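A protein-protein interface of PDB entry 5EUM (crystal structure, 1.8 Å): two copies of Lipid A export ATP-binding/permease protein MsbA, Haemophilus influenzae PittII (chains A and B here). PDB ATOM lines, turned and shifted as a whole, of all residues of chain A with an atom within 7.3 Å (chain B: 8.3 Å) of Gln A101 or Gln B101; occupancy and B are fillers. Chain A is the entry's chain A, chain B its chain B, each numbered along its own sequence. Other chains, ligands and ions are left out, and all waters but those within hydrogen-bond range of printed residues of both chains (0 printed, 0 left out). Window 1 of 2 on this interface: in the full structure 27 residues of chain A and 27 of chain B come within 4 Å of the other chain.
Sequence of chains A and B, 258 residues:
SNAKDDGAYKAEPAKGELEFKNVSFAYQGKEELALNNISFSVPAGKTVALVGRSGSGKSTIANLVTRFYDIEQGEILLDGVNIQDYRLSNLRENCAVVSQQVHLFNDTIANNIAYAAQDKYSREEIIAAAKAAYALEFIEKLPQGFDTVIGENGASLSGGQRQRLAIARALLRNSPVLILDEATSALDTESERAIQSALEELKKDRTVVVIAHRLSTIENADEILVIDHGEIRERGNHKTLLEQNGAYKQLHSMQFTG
Along chain B the printed residues that touch a printed residue of chain A span positions 101 to 181.
Among the printed residues, 6 pairs touch across the chains.
Among the printed residues, no Asp or Glu carboxylate lies within 4 Å of a Lys or Arg side-chain nitrogen of the other chain.
Printed residues of chain B within 4 Å of Gln A101: Gln B101 (3.1 Å) and Val B102 (3.7 Å).
Printed residues of chain A within 4 Å of Gln B101: Gln A101 (3.1 Å), Val A102 (3.9 Å) and His A103 (3.3 Å).
Printed residues of chain A within 4 Å of Asp B181: Asn A153.
Printed residues of chain B within 4 Å of His A103: Gln B101.
Printed residues of chain A within 4 Å of Asn B153: Asp A181 (3.5 Å).
Of the printed residues of chain B, Asp A181 touches Asn B153.
Printed residues of chain B within 4 Å of Val A102: Gln B101 (3.9 Å).
Gln B163 touches none of the printed residues of chain A.
Arg B169 touches none of the printed residues of chain A.
The nearest printed residue of chain A that does not touch Gln B101 is Leu A104 (5.1 Å).
Val B102 touches Gln A101 (O to NE2, 3.7 Å).
Val A102 touches Gln B101 (C to NE2, 3.9 Å).
Gln B101 touches His A103 (NE2 to CA, 3.3 Å).
ND2 of Asn A153 touches OD2 of Asp B181, at 3.6 Å.
Asp A181 touches Asn B153 (OD2 to ND2, 3.5 Å).
The side-chain amide nitrogen of Gln A101 is in hydrogen-bond range of the side-chain amide oxygen of Gln B101 (3.1 Å).
The backbone carbonyl oxygen (O) of Val A98 sits at hydrogen-bond distance from the backbone NH (N) of Asp A181 (2.9 Å).
NE2 of Gln A100 sits close to OD2 of Asp A181, 3.5 Å away.
The backbone carbonyl oxygen of Val B98 lies within hydrogen-bond range of the backbone NH of Asp B181 (2.8 Å).
The side-chain hydroxyl of Ser B99 sits close to the backbone NH of Gln B101.
Gln B101 touches its own counterpart, Gln A101.
Gln A101 touches Val B102, and with the chains exchanged Val A102 touches Gln B101.
His A103 touches Gln B101, but with the chains exchanged Gln A101 does not touch His B103 (4.1 Å).
Asn A153 touches Asp B181, and with the chains exchanged Asp A181 touches Asn B153.
Of the 6 pairs that touch across the chains among the printed residues, 5 have their exchanged pair printed and touching as well.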
ATOM      1  N   VAL A  98       1.971 -34.981 -24.051  1.00  0.00           N
ATOM      2  CA  VAL A  98       0.995 -34.240 -24.835  1.00  0.00           C
ATOM      3  C   VAL A  98      -0.267 -34.568 -24.053  1.00  0.00           C
ATOM      4  O   VAL A  98      -0.777 -35.692 -24.115  1.00  0.00           O
ATOM      5  CB  VAL A  98       0.868 -34.663 -26.300  1.00  0.00           C
ATOM      6  CG1 VAL A  98      -0.355 -33.999 -26.911  1.00  0.00           C
ATOM      7  CG2 VAL A  98       2.112 -34.287 -27.088  1.00  0.00           C
ATOM      8  N   SER A  99      -0.734 -33.584 -23.288  1.00  0.00           N
ATOM      9  CA  SER A  99      -1.876 -33.750 -22.391  1.00  0.00           C
ATOM     10  C   SER A  99      -3.195 -33.286 -22.981  1.00  0.00           C
ATOM     11  O   SER A  99      -3.228 -32.432 -23.864  1.00  0.00           O
ATOM     12  CB  SER A  99      -1.599 -32.974 -21.103  1.00  0.00           C
ATOM     13  OG  SER A  99      -2.659 -33.091 -20.186  1.00  0.00           O
ATOM     14  N   GLN A 100      -4.287 -33.856 -22.472  1.00  0.00           N
ATOM     15  CA  GLN A 100      -5.615 -33.493 -22.933  1.00  0.00           C
ATOM     16  C   GLN A 100      -5.690 -31.988 -23.058  1.00  0.00           C
ATOM     17  O   GLN A 100      -6.341 -31.470 -23.955  1.00  0.00           O
ATOM     18  CB  GLN A 100      -6.684 -33.939 -21.934  1.00  0.00           C
ATOM     19  CG  GLN A 100      -6.669 -35.412 -21.590  1.00  0.00           C
ATOM     20  CD  GLN A 100      -7.745 -35.763 -20.584  1.00  0.00           C
ATOM     21  OE1 GLN A 100      -8.573 -34.924 -20.234  1.00  0.00           O
ATOM     22  NE2 GLN A 100      -7.738 -36.998 -20.111  1.00  0.00           N
ATOM     23  N   GLN A 101      -5.021 -31.301 -22.134  1.00  0.00           N
ATOM     24  CA  GLN A 101      -5.000 -29.842 -22.086  1.00  0.00           C
ATOM     25  C   GLN A 101      -3.561 -29.350 -21.896  1.00  0.00           C
ATOM     26  O   GLN A 101      -2.962 -29.545 -20.836  1.00  0.00           O
ATOM     27  CB  GLN A 101      -5.861 -29.362 -20.917  1.00  0.00           C
ATOM     28  CG  GLN A 101      -5.303 -29.753 -19.555  1.00  0.00           C
ATOM     29  CD  GLN A 101      -6.221 -29.378 -18.402  1.00  0.00           C
ATOM     30  OE1 GLN A 101      -7.448 -29.391 -18.533  1.00  0.00           O
ATOM     31  NE2 GLN A 101      -5.627 -29.073 -17.252  1.00  0.00           N
ATOM     32  N   VAL A 102      -3.004 -28.713 -22.916  1.00  0.00           N
ATOM     33  CA  VAL A 102      -1.623 -28.232 -22.832  1.00  0.00           C
ATOM     34  C   VAL A 102      -1.651 -26.785 -22.338  1.00  0.00           C
ATOM     35  O   VAL A 102      -2.554 -26.035 -22.692  1.00  0.00           O
ATOM     36  CB  VAL A 102      -0.921 -28.326 -24.197  1.00  0.00           C
ATOM     37  CG1 VAL A 102      -1.532 -27.318 -25.168  1.00  0.00           C
ATOM     38  CG2 VAL A 102       0.571 -28.093 -24.041  1.00  0.00           C
ATOM     39  N   HIS A 103      -0.674 -26.390 -21.519  1.00  0.00           N
ATOM     40  CA  HIS A 103      -0.684 -25.030 -20.970  1.00  0.00           C
ATOM     41  C   HIS A 103      -0.236 -23.995 -22.003  1.00  0.00           C
ATOM     42  O   HIS A 103       0.910 -24.000 -22.413  1.00  0.00           O
ATOM     43  CB  HIS A 103       0.227 -24.953 -19.730  1.00  0.00           C
ATOM     44  CG  HIS A 103       0.202 -23.620 -19.035  1.00  0.00           C
ATOM     45  ND1 HIS A 103      -0.675 -23.331 -18.011  1.00  0.00           N
ATOM     46  CD2 HIS A 103       0.941 -22.498 -19.222  1.00  0.00           C
ATOM     47  CE1 HIS A 103      -0.475 -22.090 -17.596  1.00  0.00           C
ATOM     48  NE2 HIS A 103       0.500 -21.564 -18.314  1.00  0.00           N
ATOM     49  N   LEU A 104      -1.159 -23.148 -22.441  1.00  0.00           N
ATOM     50  CA  LEU A 104      -0.854 -22.044 -23.339  1.00  0.00           C
ATOM     51  C   LEU A 104      -1.071 -20.787 -22.525  1.00  0.00           C
ATOM     52  O   LEU A 104      -1.767 -20.800 -21.503  1.00  0.00           O
ATOM     53  CB  LEU A 104      -1.725 -22.055 -24.591  1.00  0.00           C
ATOM     54  CG  LEU A 104      -1.620 -23.262 -25.515  1.00  0.00           C
ATOM     55  CD1 LEU A 104      -2.548 -23.037 -26.691  1.00  0.00           C
ATOM     56  CD2 LEU A 104      -0.198 -23.443 -26.005  1.00  0.00           C
ATOM     57  N   ASN A 153      -5.228 -16.372 -22.802  1.00  0.00           N
ATOM     58  CA  ASN A 153      -4.383 -17.513 -22.421  1.00  0.00           C
ATOM     59  C   ASN A 153      -4.608 -18.772 -23.254  1.00  0.00           C
ATOM     60  O   ASN A 153      -4.602 -19.885 -22.721  1.00  0.00           O
ATOM     61  CB  ASN A 153      -4.513 -17.811 -20.915  1.00  0.00           C
ATOM     62  CG  ASN A 153      -3.700 -16.858 -20.062  1.00  0.00           C
ATOM     63  OD1 ASN A 153      -2.680 -16.321 -20.507  1.00  0.00           O
ATOM     64  ND2 ASN A 153      -4.113 -16.683 -18.831  1.00  0.00           N
ATOM     65  N   ALA A 166       0.675 -28.107 -29.255  1.00  0.00           N
ATOM     66  CA  ALA A 166       1.213 -29.040 -28.245  1.00  0.00           C
ATOM     67  C   ALA A 166       2.110 -30.069 -28.924  1.00  0.00           C
ATOM     68  O   ALA A 166       3.123 -30.524 -28.369  1.00  0.00           O
ATOM     69  CB  ALA A 166       0.067 -29.744 -27.489  1.00  0.00           C
ATOM     70  N   ASP A 181      -1.841 -38.391 -24.437  1.00  0.00           N
ATOM     71  CA  ASP A 181      -3.132 -38.615 -23.808  1.00  0.00           C
ATOM     72  C   ASP A 181      -4.210 -38.180 -24.810  1.00  0.00           C
ATOM     73  O   ASP A 181      -4.383 -36.974 -25.081  1.00  0.00           O
ATOM     74  CB  ASP A 181      -3.171 -37.798 -22.495  1.00  0.00           C
ATOM     75  CG  ASP A 181      -4.371 -38.120 -21.600  1.00  0.00           C
ATOM     76  OD1 ASP A 181      -5.312 -38.821 -22.058  1.00  0.00           O
ATOM     77  OD2 ASP A 181      -4.350 -37.664 -20.408  1.00  0.00           O
ATOM     78  N   VAL B  97      -4.391 -19.585  -8.038  1.00  0.00           N
ATOM     79  CA  VAL B  97      -4.978 -19.348  -9.359  1.00  0.00           C
ATOM     80  C   VAL B  97      -6.103 -20.337  -9.567  1.00  0.00           C
ATOM     81  O   VAL B  97      -5.947 -21.526  -9.253  1.00  0.00           O
ATOM     82  CB  VAL B  97      -3.935 -19.498 -10.472  1.00  0.00           C
ATOM     83  CG1 VAL B  97      -4.560 -19.219 -11.849  1.00  0.00           C
ATOM     84  CG2 VAL B  97      -2.759 -18.582 -10.216  1.00  0.00           C
ATOM     85  N   VAL B  98      -7.223 -19.861 -10.102  1.00  0.00           N
ATOM     86  CA  VAL B  98      -8.334 -20.721 -10.491  1.00  0.00           C
ATOM     87  C   VAL B  98      -8.558 -20.466 -11.977  1.00  0.00           C
ATOM     88  O   VAL B  98      -8.802 -19.335 -12.382  1.00  0.00           O
ATOM     89  CB  VAL B  98      -9.645 -20.444  -9.745  1.00  0.00           C
ATOM     90  CG1 VAL B  98     -10.788 -21.172 -10.439  1.00  0.00           C
ATOM     91  CG2 VAL B  98      -9.550 -20.881  -8.291  1.00  0.00           C
ATOM     92  N   SER B  99      -8.455 -21.507 -12.793  1.00  0.00           N
ATOM     93  CA  SER B  99      -8.662 -21.345 -14.230  1.00  0.00           C
ATOM     94  C   SER B  99      -9.124 -22.647 -14.860  1.00  0.00           C
ATOM     95  O   SER B  99      -8.977 -23.708 -14.249  1.00  0.00           O
ATOM     96  CB  SER B  99      -7.371 -20.882 -14.903  1.00  0.00           C
ATOM     97  OG  SER B  99      -6.327 -21.826 -14.733  1.00  0.00           O
ATOM     98  N   GLN B 100      -9.667 -22.584 -16.077  1.00  0.00           N
ATOM     99  CA  GLN B 100     -10.123 -23.819 -16.713  1.00  0.00           C
ATOM    100  C   GLN B 100      -8.943 -24.776 -16.783  1.00  0.00           C
ATOM    101  O   GLN B 100      -9.107 -25.995 -16.885  1.00  0.00           O
ATOM    102  CB  GLN B 100     -10.760 -23.593 -18.095  1.00  0.00           C
ATOM    103  CG  GLN B 100      -9.879 -23.006 -19.200  1.00  0.00           C
ATOM    104  CD  GLN B 100      -9.743 -21.494 -19.146  1.00  0.00           C
ATOM    105  OE1 GLN B 100      -9.749 -20.887 -18.082  1.00  0.00           O
ATOM    106  NE2 GLN B 100      -9.607 -20.877 -20.318  1.00  0.00           N
ATOM    107  N   GLN B 101      -7.746 -24.210 -16.692  1.00  0.00           N
ATOM    108  CA  GLN B 101      -6.519 -24.991 -16.731  1.00  0.00           C
ATOM    109  C   GLN B 101      -6.213 -25.629 -15.369  1.00  0.00           C
ATOM    110  O   GLN B 101      -5.050 -25.763 -14.988  1.00  0.00           O
ATOM    111  CB  GLN B 101      -5.359 -24.092 -17.168  1.00  0.00           C
ATOM    112  CG  GLN B 101      -4.007 -24.778 -17.255  1.00  0.00           C
ATOM    113  CD  GLN B 101      -3.956 -25.887 -18.293  1.00  0.00           C
ATOM    114  OE1 GLN B 101      -4.988 -26.397 -18.734  1.00  0.00           O
ATOM    115  NE2 GLN B 101      -2.748 -26.273 -18.682  1.00  0.00           N
ATOM    116  N   VAL B 102      -7.253 -26.019 -14.634  1.00  0.00           N
ATOM    117  CA  VAL B 102      -7.054 -26.656 -13.328  1.00  0.00           C
ATOM    118  C   VAL B 102      -6.662 -28.122 -13.548  1.00  0.00           C
ATOM    119  O   VAL B 102      -7.436 -28.911 -14.084  1.00  0.00           O
ATOM    120  CB  VAL B 102      -8.313 -26.594 -12.443  1.00  0.00           C
ATOM    121  CG1 VAL B 102      -9.416 -27.468 -13.029  1.00  0.00           C
ATOM    122  CG2 VAL B 102      -7.979 -27.044 -11.027  1.00  0.00           C
ATOM    123  N   HIS B 103      -5.456 -28.473 -13.119  1.00  0.00           N
ATOM    124  CA  HIS B 103      -4.915 -29.825 -13.300  1.00  0.00           C
ATOM    125  C   HIS B 103      -5.542 -30.856 -12.359  1.00  0.00           C
ATOM    126  O   HIS B 103      -5.383 -30.767 -11.153  1.00  0.00           O
ATOM    127  CB  HIS B 103      -3.383 -29.810 -13.117  1.00  0.00           C
ATOM    128  CG  HIS B 103      -2.717 -31.128 -13.403  1.00  0.00           C
ATOM    129  ND1 HIS B 103      -2.311 -31.500 -14.669  1.00  0.00           N
ATOM    130  CD2 HIS B 103      -2.382 -32.159 -12.586  1.00  0.00           C
ATOM    131  CE1 HIS B 103      -1.762 -32.704 -14.620  1.00  0.00           C
ATOM    132  NE2 HIS B 103      -1.791 -33.125 -13.368  1.00  0.00           N
ATOM    133  N   LEU B 104      -6.274 -31.811 -12.932  1.00  0.00           N
ATOM    134  CA  LEU B 104      -6.839 -32.933 -12.193  1.00  0.00           C
ATOM    135  C   LEU B 104      -6.113 -34.164 -12.701  1.00  0.00           C
ATOM    136  O   LEU B 104      -5.508 -34.151 -13.785  1.00  0.00           O
ATOM    137  CB  LEU B 104      -8.346 -33.065 -12.380  1.00  0.00           C
ATOM    138  CG  LEU B 104      -9.252 -31.961 -11.842  1.00  0.00           C
ATOM    139  CD1 LEU B 104     -10.689 -32.345 -12.123  1.00  0.00           C
ATOM    140  CD2 LEU B 104      -9.061 -31.771 -10.344  1.00  0.00           C
ATOM    141  N   PHE B 105      -6.189 -35.236 -11.936  1.00  0.00           N
ATOM    142  CA  PHE B 105      -5.429 -36.430 -12.241  1.00  0.00           C
ATOM    143  C   PHE B 105      -6.051 -37.639 -11.597  1.00  0.00           C
ATOM    144  O   PHE B 105      -6.800 -37.512 -10.615  1.00  0.00           O
ATOM    145  CB  PHE B 105      -4.009 -36.232 -11.690  1.00  0.00           C
ATOM    146  CG  PHE B 105      -3.986 -35.699 -10.275  1.00  0.00           C
ATOM    147  CD1 PHE B 105      -4.013 -34.319 -10.024  1.00  0.00           C
ATOM    148  CD2 PHE B 105      -3.984 -36.562  -9.196  1.00  0.00           C
ATOM    149  CE1 PHE B 105      -4.008 -33.835  -8.715  1.00  0.00           C
ATOM    150  CE2 PHE B 105      -3.975 -36.078  -7.892  1.00  0.00           C
ATOM    151  CZ  PHE B 105      -3.989 -34.721  -7.652  1.00  0.00           C
ATOM    152  N   ASN B 153      -7.957 -38.932 -16.009  1.00  0.00           N
ATOM    153  CA  ASN B 153      -7.305 -37.714 -15.508  1.00  0.00           C
ATOM    154  C   ASN B 153      -8.249 -36.515 -15.360  1.00  0.00           C
ATOM    155  O   ASN B 153      -7.866 -35.367 -15.625  1.00  0.00           O
ATOM    156  CB  ASN B 153      -6.076 -37.360 -16.365  1.00  0.00           C
ATOM    157  CG  ASN B 153      -4.864 -38.187 -16.008  1.00  0.00           C
ATOM    158  OD1 ASN B 153      -4.728 -38.664 -14.869  1.00  0.00           O
ATOM    159  ND2 ASN B 153      -3.960 -38.330 -16.957  1.00  0.00           N
ATOM    160  N   GLY B 154      -9.486 -36.796 -14.974  1.00  0.00           N
ATOM    161  CA  GLY B 154     -10.490 -35.755 -14.795  1.00  0.00           C
ATOM    162  C   GLY B 154     -11.651 -35.735 -15.769  1.00  0.00           C
ATOM    163  O   GLY B 154     -12.690 -35.122 -15.476  1.00  0.00           O
ATOM    164  N   ALA B 155     -11.520 -36.403 -16.905  1.00  0.00           N
ATOM    165  CA  ALA B 155     -12.606 -36.385 -17.904  1.00  0.00           C
ATOM    166  C   ALA B 155     -13.870 -37.118 -17.418  1.00  0.00           C
ATOM    167  O   ALA B 155     -14.939 -36.927 -17.998  1.00  0.00           O
ATOM    168  CB  ALA B 155     -12.141 -36.947 -19.239  1.00  0.00           C
ATOM    169  N   ARG B 162     -15.658 -30.072 -12.298  1.00  0.00           N
ATOM    170  CA  ARG B 162     -14.226 -29.742 -12.290  1.00  0.00           C
ATOM    171  C   ARG B 162     -13.959 -28.311 -11.803  1.00  0.00           C
ATOM    172  O   ARG B 162     -13.002 -28.102 -11.046  1.00  0.00           O
ATOM    173  CB  ARG B 162     -13.570 -30.003 -13.674  1.00  0.00           C
ATOM    174  CG  ARG B 162     -13.506 -31.484 -14.020  1.00  0.00           C
ATOM    175  CD  ARG B 162     -12.615 -31.762 -15.235  1.00  0.00           C
ATOM    176  NE  ARG B 162     -13.091 -31.097 -16.444  1.00  0.00           N
ATOM    177  CZ  ARG B 162     -13.931 -31.621 -17.346  1.00  0.00           C
ATOM    178  NH1 ARG B 162     -14.283 -30.900 -18.410  1.00  0.00           N
ATOM    179  NH2 ARG B 162     -14.424 -32.853 -17.211  1.00  0.00           N
ATOM    180  N   GLN B 163     -14.800 -27.340 -12.190  1.00  0.00           N
ATOM    181  CA  GLN B 163     -14.631 -25.942 -11.721  1.00  0.00           C
ATOM    182  C   GLN B 163     -14.827 -25.849 -10.196  1.00  0.00           C
ATOM    183  O   GLN B 163     -14.113 -25.125  -9.513  1.00  0.00           O
ATOM    184  CB  GLN B 163     -15.604 -24.956 -12.394  1.00  0.00           C
ATOM    185  CG  GLN B 163     -15.439 -24.788 -13.907  1.00  0.00           C
ATOM    186  CD  GLN B 163     -16.379 -23.737 -14.515  1.00  0.00           C
ATOM    187  OE1 GLN B 163     -16.648 -22.687 -13.924  1.00  0.00           O
ATOM    188  NE2 GLN B 163     -16.855 -24.010 -15.717  1.00  0.00           N
ATOM    189  N   ALA B 166     -11.887 -27.102  -8.330  1.00  0.00           N
ATOM    190  CA  ALA B 166     -10.823 -26.086  -8.396  1.00  0.00           C
ATOM    191  C   ALA B 166     -11.056 -25.009  -7.345  1.00  0.00           C
ATOM    192  O   ALA B 166     -10.110 -24.457  -6.750  1.00  0.00           O
ATOM    193  CB  ALA B 166     -10.767 -25.470  -9.807  1.00  0.00           C
ATOM    194  N   ARG B 169     -10.286 -26.633  -3.933  1.00  0.00           N
ATOM    195  CA  ARG B 169      -8.844 -26.686  -3.785  1.00  0.00           C
ATOM    196  C   ARG B 169      -8.328 -25.312  -3.312  1.00  0.00           C
ATOM    197  O   ARG B 169      -7.472 -25.219  -2.404  1.00  0.00           O
ATOM    198  CB  ARG B 169      -8.200 -27.132  -5.130  1.00  0.00           C
ATOM    199  CG  ARG B 169      -6.690 -27.279  -5.114  1.00  0.00           C
ATOM    200  CD  ARG B 169      -6.149 -27.585  -6.510  1.00  0.00           C
ATOM    201  NE  ARG B 169      -6.361 -28.973  -6.902  1.00  0.00           N
ATOM    202  CZ  ARG B 169      -6.054 -29.482  -8.098  1.00  0.00           C
ATOM    203  NH1 ARG B 169      -5.552 -28.708  -9.054  1.00  0.00           N
ATOM    204  NH2 ARG B 169      -6.276 -30.767  -8.352  1.00  0.00           N
ATOM    205  N   ASP B 181      -9.698 -16.825 -13.373  1.00  0.00           N
ATOM    206  CA  ASP B 181      -9.764 -16.670 -14.820  1.00  0.00           C
ATOM    207  C   ASP B 181     -11.115 -17.239 -15.267  1.00  0.00           C
ATOM    208  O   ASP B 181     -11.330 -18.475 -15.235  1.00  0.00           O
ATOM    209  CB  ASP B 181      -8.548 -17.416 -15.433  1.00  0.00           C
ATOM    210  CG  ASP B 181      -8.354 -17.173 -16.934  1.00  0.00           C
ATOM    211  OD1 ASP B 181      -9.234 -16.537 -17.574  1.00  0.00           O
ATOM    212  OD2 ASP B 181      -7.275 -17.616 -17.471  1.00  0.00           O
